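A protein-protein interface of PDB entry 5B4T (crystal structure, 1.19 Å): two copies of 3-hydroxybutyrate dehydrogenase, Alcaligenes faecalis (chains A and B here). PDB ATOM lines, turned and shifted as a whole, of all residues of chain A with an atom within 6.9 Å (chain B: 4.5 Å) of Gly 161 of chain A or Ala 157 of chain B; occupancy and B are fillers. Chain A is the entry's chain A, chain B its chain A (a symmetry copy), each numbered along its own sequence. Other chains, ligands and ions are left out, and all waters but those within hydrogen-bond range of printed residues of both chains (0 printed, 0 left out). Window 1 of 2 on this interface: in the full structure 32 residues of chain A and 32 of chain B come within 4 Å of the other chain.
Ala 157 of chain A touches Gly 161 of chain B, and with the chains exchanged Gly 161 of chain A touches Ala 157 of chain B. His 160 of chain A touches its own counterpart, His 160 of chain B. Of the 10 pairs that touch across the chains among the printed residues, 3 have their exchanged pair printed and touching as well.
Hydrophobic or aromatic side chains of chain B within 4 Å of the printed part of chain A: Trp 107, Val 156, Ala 157 and His 160. Among the printed residues, no Asp or Glu carboxylate lies within 4 Å of a Lys or Arg side-chain nitrogen of the other chain.
A ring nitrogen (ND1) of His 160 of chain A is in hydrogen-bond range of the backbone carbonyl oxygen (O) of His 144 of chain A (2.9 Å). The backbone carbonyl oxygen of Val 156 of chain B sits at hydrogen-bond distance from a ring nitrogen (ND1) of His 160 of chain B. A ring nitrogen (ND1) of His 160 of chain A is in hydrogen-bond range of the backbone carbonyl oxygen (O) of Val 156 of chain A, at 3.0 Å. O of Gly 145 of chain A sits close to ND1 of His 160 of chain A (3.4 Å).
Among the printed residues, pairs that only touch across the chains: Leu 115 of chain A with Trp 107 of chain B (3.99 Å), Ala 157 of chain A with Gly 161 of chain B (3.4 Å), His 160 of chain A with His 160 of chain B (3.2 Å), Gly 161 of chain A with Ala 157 of chain B (3.4 Å), Gly 164 of chain A with Val 156 of chain B (3.6 Å), Gly 164 of chain A with His 160 of chain B (3.5 Å), Leu 165 of chain A with Ser 153 of chain B (3.7 Å), Val 168 of chain A with Ser 153 of chain B (3.8 Å) and Val 168 of chain A with Val 156 of chain B (3.6 Å).
Of chain B, only Ala 157 comes within 4 Å of Gly 161 of chain A. Printed residues of chain A within 4 Å of Ala 157 of chain B: Gly 161. Of the printed residues of chain B, Leu 115 of chain A touches Trp 107 (3.99 Å). Printed residues of chain B within 4 Å of Gly 164 of chain A: Val 156 (3.6 Å) and His 160 (3.5 Å). Ala 158 of chain A touches none of the printed residues of chain B. Ala 158 of chain B touches none of the printed residues of chain A. The nearest residue of chain A that does not touch Ala 157 of chain B is Leu 115 of chain A (4.3 Å).
The side-chain amino group (NZ) of Lys 167 of chain A lies within hydrogen-bond range of a ring nitrogen (NE2) of His 160 of chain B, 2.9 Å away.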
ATOM      1  N   ASN A 114      18.763  15.044   4.820  1.00  0.00           N
ATOM      2  CA  ASN A 114      19.737  14.177   4.215  1.00  0.00           C
ATOM      3  C   ASN A 114      20.741  14.921   3.333  1.00  0.00           C
ATOM      4  O   ASN A 114      21.795  14.359   3.002  1.00  0.00           O
ATOM      5  CB  ASN A 114      19.061  13.092   3.385  1.00  0.00           C
ATOM      6  CG  ASN A 114      18.220  12.120   4.208  1.00  0.00           C
ATOM      7  OD1 ASN A 114      17.730  12.423   5.301  1.00  0.00           O
ATOM      8  ND2 ASN A 114      17.989  10.947   3.655  1.00  0.00           N
ATOM      9  N   LEU A 115      20.391  16.099   2.840  1.00  0.00           N
ATOM     10  CA  LEU A 115      21.288  16.866   1.994  1.00  0.00           C
ATOM     11  C   LEU A 115      21.662  18.203   2.633  1.00  0.00           C
ATOM     12  O   LEU A 115      22.818  18.468   2.861  1.00  0.00           O
ATOM     13  CB  LEU A 115      20.712  17.032   0.585  1.00  0.00           C
ATOM     14  CG  LEU A 115      21.535  17.890  -0.377  1.00  0.00           C
ATOM     15  CD1 LEU A 115      22.953  17.353  -0.510  1.00  0.00           C
ATOM     16  CD2 LEU A 115      20.816  17.993  -1.713  1.00  0.00           C
ATOM     17  N   HIS A 144      22.693   4.354  -2.711  1.00  0.00           N
ATOM     18  CA  HIS A 144      21.742   5.256  -3.388  1.00  0.00           C
ATOM     19  C   HIS A 144      22.255   6.650  -3.649  1.00  0.00           C
ATOM     20  O   HIS A 144      21.543   7.458  -4.254  1.00  0.00           O
ATOM     21  CB  HIS A 144      20.432   5.299  -2.618  1.00  0.00           C
ATOM     22  CG  HIS A 144      19.610   4.073  -2.815  1.00  0.00           C
ATOM     23  ND1 HIS A 144      19.093   3.345  -1.765  1.00  0.00           N
ATOM     24  CD2 HIS A 144      19.334   3.379  -3.930  1.00  0.00           C
ATOM     25  CE1 HIS A 144      18.435   2.311  -2.258  1.00  0.00           C
ATOM     26  NE2 HIS A 144      18.560   2.303  -3.565  1.00  0.00           N
ATOM     27  N   GLY A 145      23.516   6.907  -3.351  1.00  0.00           N
ATOM     28  CA  GLY A 145      24.228   8.076  -3.843  1.00  0.00           C
ATOM     29  C   GLY A 145      24.930   7.834  -5.161  1.00  0.00           C
ATOM     30  O   GLY A 145      25.442   8.774  -5.759  1.00  0.00           O
ATOM     31  N   TYR A 155      15.224  10.385  -1.558  1.00  0.00           N
ATOM     32  CA  TYR A 155      16.395   9.838  -0.902  1.00  0.00           C
ATOM     33  C   TYR A 155      17.574   9.674  -1.877  1.00  0.00           C
ATOM     34  O   TYR A 155      18.690  10.028  -1.556  1.00  0.00           O
ATOM     35  CB  TYR A 155      16.018   8.509  -0.264  1.00  0.00           C
ATOM     36  CG  TYR A 155      17.098   7.876   0.583  1.00  0.00           C
ATOM     37  CD1 TYR A 155      17.986   6.954   0.040  1.00  0.00           C
ATOM     38  CD2 TYR A 155      17.128   8.066   1.959  1.00  0.00           C
ATOM     39  CE1 TYR A 155      18.911   6.289   0.833  1.00  0.00           C
ATOM     40  CE2 TYR A 155      18.069   7.442   2.745  1.00  0.00           C
ATOM     41  CZ  TYR A 155      18.905   6.490   2.181  1.00  0.00           C
ATOM     42  OH  TYR A 155      19.830   5.828   2.957  1.00  0.00           O
ATOM     43  N   VAL A 156      17.299   9.106  -3.050  1.00  0.00           N
ATOM     44  CA  VAL A 156      18.312   8.966  -4.073  1.00  0.00           C
ATOM     45  C   VAL A 156      18.834  10.315  -4.519  1.00  0.00           C
ATOM     46  O   VAL A 156      20.047  10.522  -4.656  1.00  0.00           O
ATOM     47  CB  VAL A 156      17.790   8.160  -5.276  1.00  0.00           C
ATOM     48  CG1 VAL A 156      18.813   8.168  -6.382  1.00  0.00           C
ATOM     49  CG2 VAL A 156      17.474   6.717  -4.882  1.00  0.00           C
ATOM     50  N   ALA A 157      17.943  11.275  -4.719  1.00  0.00           N
ATOM     51  CA  ALA A 157      18.373  12.623  -5.079  1.00  0.00           C
ATOM     52  C   ALA A 157      19.260  13.218  -3.995  1.00  0.00           C
ATOM     53  O   ALA A 157      20.341  13.754  -4.271  1.00  0.00           O
ATOM     54  CB  ALA A 157      17.173  13.502  -5.357  1.00  0.00           C
ATOM     55  N   ALA A 158      18.831  13.104  -2.748  1.00  0.00           N
ATOM     56  CA  ALA A 158      19.595  13.654  -1.643  1.00  0.00           C
ATOM     57  C   ALA A 158      20.985  13.019  -1.533  1.00  0.00           C
ATOM     58  O   ALA A 158      21.973  13.706  -1.319  1.00  0.00           O
ATOM     59  CB  ALA A 158      18.842  13.479  -0.332  1.00  0.00           C
ATOM     60  N   LYS A 159      21.026  11.692  -1.603  1.00  0.00           N
ATOM     61  CA  LYS A 159      22.266  10.962  -1.437  1.00  0.00           C
ATOM     62  C   LYS A 159      23.221  11.212  -2.592  1.00  0.00           C
ATOM     63  O   LYS A 159      24.417  11.339  -2.391  1.00  0.00           O
ATOM     64  CB  LYS A 159      22.013   9.466  -1.246  1.00  0.00           C
ATOM     65  CG  LYS A 159      21.284   9.134   0.046  1.00  0.00           C
ATOM     66  CD  LYS A 159      22.053   9.517   1.283  1.00  0.00           C
ATOM     67  CE  LYS A 159      21.473   8.921   2.553  1.00  0.00           C
ATOM     68  NZ  LYS A 159      22.273   9.304   3.755  1.00  0.00           N
ATOM     69  N   HIS A 160      22.702  11.281  -3.814  1.00  0.00           N
ATOM     70  CA  HIS A 160      23.533  11.724  -4.940  1.00  0.00           C
ATOM     71  C   HIS A 160      24.085  13.131  -4.654  1.00  0.00           C
ATOM     72  O   HIS A 160      25.278  13.418  -4.888  1.00  0.00           O
ATOM     73  CB  HIS A 160      22.754  11.725  -6.252  1.00  0.00           C
ATOM     74  CG  HIS A 160      22.740  10.412  -6.957  1.00  0.00           C
ATOM     75  ND1 HIS A 160      22.157   9.278  -6.441  1.00  0.00           N
ATOM     76  CD2 HIS A 160      23.219  10.062  -8.178  1.00  0.00           C
ATOM     77  CE1 HIS A 160      22.303   8.278  -7.308  1.00  0.00           C
ATOM     78  NE2 HIS A 160      22.943   8.729  -8.370  1.00  0.00           N
ATOM     79  N   GLY A 161      23.239  14.014  -4.141  1.00  0.00           N
ATOM     80  CA  GLY A 161      23.657  15.335  -3.743  1.00  0.00           C
ATOM     81  C   GLY A 161      24.779  15.338  -2.746  1.00  0.00           C
ATOM     82  O   GLY A 161      25.702  16.122  -2.850  1.00  0.00           O
ATOM     83  N   VAL A 162      24.695  14.462  -1.754  1.00  0.00           N
ATOM     84  CA  VAL A 162      25.736  14.327  -0.760  1.00  0.00           C
ATOM     85  C   VAL A 162      27.057  13.906  -1.378  1.00  0.00           C
ATOM     86  O   VAL A 162      28.097  14.427  -1.038  1.00  0.00           O
ATOM     87  CB  VAL A 162      25.339  13.345   0.353  1.00  0.00           C
ATOM     88  CG1 VAL A 162      26.535  13.050   1.243  1.00  0.00           C
ATOM     89  CG2 VAL A 162      24.186  13.894   1.172  1.00  0.00           C
ATOM     90  N   VAL A 163      27.006  12.978  -2.314  1.00  0.00           N
ATOM     91  CA  VAL A 163      28.218  12.588  -3.019  1.00  0.00           C
ATOM     92  C   VAL A 163      28.836  13.752  -3.767  1.00  0.00           C
ATOM     93  O   VAL A 163      30.048  13.989  -3.675  1.00  0.00           O
ATOM     94  CB  VAL A 163      27.907  11.395  -3.931  1.00  0.00           C
ATOM     95  CG1 VAL A 163      29.052  11.114  -4.883  1.00  0.00           C
ATOM     96  CG2 VAL A 163      27.570  10.163  -3.115  1.00  0.00           C
ATOM     97  N   GLY A 164      28.017  14.547  -4.440  1.00  0.00           N
ATOM     98  CA  GLY A 164      28.529  15.754  -5.095  1.00  0.00           C
ATOM     99  C   GLY A 164      29.109  16.750  -4.133  1.00  0.00           C
ATOM    100  O   GLY A 164      30.172  17.325  -4.387  1.00  0.00           O
ATOM    101  N   LEU A 165      28.397  17.001  -3.046  1.00  0.00           N
ATOM    102  CA  LEU A 165      28.852  17.951  -2.067  1.00  0.00           C
ATOM    103  C   LEU A 165      30.166  17.507  -1.430  1.00  0.00           C
ATOM    104  O   LEU A 165      31.047  18.343  -1.171  1.00  0.00           O
ATOM    105  CB  LEU A 165      27.773  18.096  -1.012  1.00  0.00           C
ATOM    106  CG  LEU A 165      28.057  19.034   0.130  1.00  0.00           C
ATOM    107  CD1 LEU A 165      28.310  20.460  -0.330  1.00  0.00           C
ATOM    108  CD2 LEU A 165      26.877  18.950   1.099  1.00  0.00           C
ATOM    109  N   THR A 166      30.335  16.211  -1.220  1.00  0.00           N
ATOM    110  CA  THR A 166      31.556  15.652  -0.693  1.00  0.00           C
ATOM    111  C   THR A 166      32.741  16.005  -1.598  1.00  0.00           C
ATOM    112  O   THR A 166      33.818  16.399  -1.132  1.00  0.00           O
ATOM    113  CB  THR A 166      31.419  14.137  -0.611  1.00  0.00           C
ATOM    114  OG1 THR A 166      30.404  13.828   0.357  1.00  0.00           O
ATOM    115  CG2 THR A 166      32.699  13.479  -0.198  1.00  0.00           C
ATOM    116  N   LYS A 167      32.542  15.849  -2.898  1.00  0.00           N
ATOM    117  CA  LYS A 167      33.568  16.201  -3.865  1.00  0.00           C
ATOM    118  C   LYS A 167      33.958  17.662  -3.806  1.00  0.00           C
ATOM    119  O   LYS A 167      35.133  18.003  -3.827  1.00  0.00           O
ATOM    120  CB  LYS A 167      33.120  15.809  -5.265  1.00  0.00           C
ATOM    121  CG  LYS A 167      32.877  14.347  -5.491  1.00  0.00           C
ATOM    122  CD  LYS A 167      32.209  14.123  -6.861  1.00  0.00           C
ATOM    123  CE  LYS A 167      31.587  12.741  -6.973  1.00  0.00           C
ATOM    124  NZ  LYS A 167      30.898  12.559  -8.278  1.00  0.00           N
ATOM    125  N   VAL A 168      32.966  18.543  -3.773  1.00  0.00           N
ATOM    126  CA  VAL A 168      33.260  19.972  -3.697  1.00  0.00           C
ATOM    127  C   VAL A 168      34.036  20.293  -2.420  1.00  0.00           C
ATOM    128  O   VAL A 168      35.030  21.027  -2.437  1.00  0.00           O
ATOM    129  CB  VAL A 168      31.965  20.825  -3.766  1.00  0.00           C
ATOM    130  CG1 VAL A 168      32.294  22.298  -3.546  1.00  0.00           C
ATOM    131  CG2 VAL A 168      31.284  20.678  -5.102  1.00  0.00           C
ATOM    132  N   TRP B 107      21.994  28.755  -1.449  1.00  0.00           N
ATOM    133  CA  TRP B 107      21.841  27.296  -1.353  1.00  0.00           C
ATOM    134  C   TRP B 107      20.382  26.927  -1.541  1.00  0.00           C
ATOM    135  O   TRP B 107      20.026  26.105  -2.387  1.00  0.00           O
ATOM    136  CB  TRP B 107      22.373  26.778  -0.015  1.00  0.00           C
ATOM    137  CG  TRP B 107      22.008  25.342   0.239  1.00  0.00           C
ATOM    138  CD1 TRP B 107      20.909  24.888   0.877  1.00  0.00           C
ATOM    139  CD2 TRP B 107      22.763  24.186  -0.118  1.00  0.00           C
ATOM    140  NE1 TRP B 107      20.879  23.509   0.857  1.00  0.00           N
ATOM    141  CE2 TRP B 107      21.982  23.071   0.187  1.00  0.00           C
ATOM    142  CE3 TRP B 107      24.004  23.981  -0.706  1.00  0.00           C
ATOM    143  CZ2 TRP B 107      22.420  21.763  -0.025  1.00  0.00           C
ATOM    144  CZ3 TRP B 107      24.416  22.651  -0.928  1.00  0.00           C
ATOM    145  CH2 TRP B 107      23.617  21.600  -0.622  1.00  0.00           C
ATOM    146  N   SER B 153      29.277  24.357  -4.493  1.00  0.00           N
ATOM    147  CA  SER B 153      28.637  23.338  -3.654  1.00  0.00           C
ATOM    148  C   SER B 153      27.165  23.140  -3.972  1.00  0.00           C
ATOM    149  O   SER B 153      26.731  21.995  -4.191  1.00  0.00           O
ATOM    150  CB  SER B 153      28.799  23.650  -2.186  1.00  0.00           C
ATOM    151  OG  SER B 153      28.359  24.949  -1.869  1.00  0.00           O
ATOM    152  N   ALA B 154      26.376  24.207  -3.986  1.00  0.00           N
ATOM    153  CA  ALA B 154      24.942  24.033  -4.155  1.00  0.00           C
ATOM    154  C   ALA B 154      24.616  23.459  -5.540  1.00  0.00           C
ATOM    155  O   ALA B 154      23.748  22.620  -5.702  1.00  0.00           O
ATOM    156  CB  ALA B 154      24.215  25.354  -3.958  1.00  0.00           C
ATOM    157  N   TYR B 155      25.271  24.000  -6.547  1.00  0.00           N
ATOM    158  CA  TYR B 155      25.007  23.614  -7.920  1.00  0.00           C
ATOM    159  C   TYR B 155      25.410  22.154  -8.193  1.00  0.00           C
ATOM    160  O   TYR B 155      24.666  21.417  -8.808  1.00  0.00           O
ATOM    161  CB  TYR B 155      25.746  24.572  -8.844  1.00  0.00           C
ATOM    162  CG  TYR B 155      25.460  24.390 -10.316  1.00  0.00           C
ATOM    163  CD1 TYR B 155      26.263  23.575 -11.108  1.00  0.00           C
ATOM    164  CD2 TYR B 155      24.496  25.159 -10.955  1.00  0.00           C
ATOM    165  CE1 TYR B 155      26.071  23.486 -12.479  1.00  0.00           C
ATOM    166  CE2 TYR B 155      24.274  25.046 -12.308  1.00  0.00           C
ATOM    167  CZ  TYR B 155      25.124  24.264 -13.076  1.00  0.00           C
ATOM    168  OH  TYR B 155      24.941  24.165 -14.436  1.00  0.00           O
ATOM    169  N   VAL B 156      26.606  21.776  -7.747  1.00  0.00           N
ATOM    170  CA  VAL B 156      27.060  20.409  -7.881  1.00  0.00           C
ATOM    171  C   VAL B 156      26.156  19.452  -7.134  1.00  0.00           C
ATOM    172  O   VAL B 156      25.771  18.395  -7.650  1.00  0.00           O
ATOM    173  CB  VAL B 156      28.520  20.252  -7.417  1.00  0.00           C
ATOM    174  CG1 VAL B 156      28.907  18.796  -7.424  1.00  0.00           C
ATOM    175  CG2 VAL B 156      29.474  21.039  -8.315  1.00  0.00           C
ATOM    176  N   ALA B 157      25.763  19.811  -5.920  1.00  0.00           N
ATOM    177  CA  ALA B 157      24.832  18.978  -5.165  1.00  0.00           C
ATOM    178  C   ALA B 157      23.513  18.828  -5.908  1.00  0.00           C
ATOM    179  O   ALA B 157      22.990  17.718  -6.072  1.00  0.00           O
ATOM    180  CB  ALA B 157      24.625  19.544  -3.777  1.00  0.00           C
ATOM    181  N   ALA B 158      22.973  19.935  -6.391  1.00  0.00           N
ATOM    182  CA  ALA B 158      21.707  19.902  -7.100  1.00  0.00           C
ATOM    183  C   ALA B 158      21.778  19.036  -8.362  1.00  0.00           C
ATOM    184  O   ALA B 158      20.874  18.263  -8.643  1.00  0.00           O
ATOM    185  CB  ALA B 158      21.259  21.310  -7.463  1.00  0.00           C
ATOM    186  N   LYS B 159      22.827  19.243  -9.152  1.00  0.00           N
ATOM    187  CA  LYS B 159      22.975  18.548 -10.414  1.00  0.00           C
ATOM    188  C   LYS B 159      23.222  17.064 -10.207  1.00  0.00           C
ATOM    189  O   LYS B 159      22.704  16.240 -10.943  1.00  0.00           O
ATOM    190  CB  LYS B 159      24.074  19.175 -11.272  1.00  0.00           C
ATOM    191  CG  LYS B 159      23.753  20.586 -11.734  1.00  0.00           C
ATOM    192  CD  LYS B 159      22.535  20.664 -12.618  1.00  0.00           C
ATOM    193  CE  LYS B 159      22.390  22.004 -13.316  1.00  0.00           C
ATOM    194  NZ  LYS B 159      21.186  22.037 -14.199  1.00  0.00           N
ATOM    195  N   HIS B 160      24.021  16.707  -9.206  1.00  0.00           N
ATOM    196  CA  HIS B 160      24.135  15.294  -8.825  1.00  0.00           C
ATOM    197  C   HIS B 160      22.747  14.745  -8.451  1.00  0.00           C
ATOM    198  O   HIS B 160      22.363  13.627  -8.856  1.00  0.00           O
ATOM    199  CB  HIS B 160      25.105  15.097  -7.663  1.00  0.00           C
ATOM    200  CG  HIS B 160      26.531  14.959  -8.072  1.00  0.00           C
ATOM    201  ND1 HIS B 160      27.244  15.959  -8.691  1.00  0.00           N
ATOM    202  CD2 HIS B 160      27.398  13.928  -7.913  1.00  0.00           C
ATOM    203  CE1 HIS B 160      28.486  15.535  -8.918  1.00  0.00           C
ATOM    204  NE2 HIS B 160      28.603  14.305  -8.454  1.00  0.00           N
ATOM    205  N   GLY B 161      21.981  15.518  -7.693  1.00  0.00           N
ATOM    206  CA  GLY B 161      20.627  15.158  -7.353  1.00  0.00           C
ATOM    207  C   GLY B 161      19.753  14.900  -8.546  1.00  0.00           C
ATOM    208  O   GLY B 161      18.980  13.962  -8.559  1.00  0.00           O
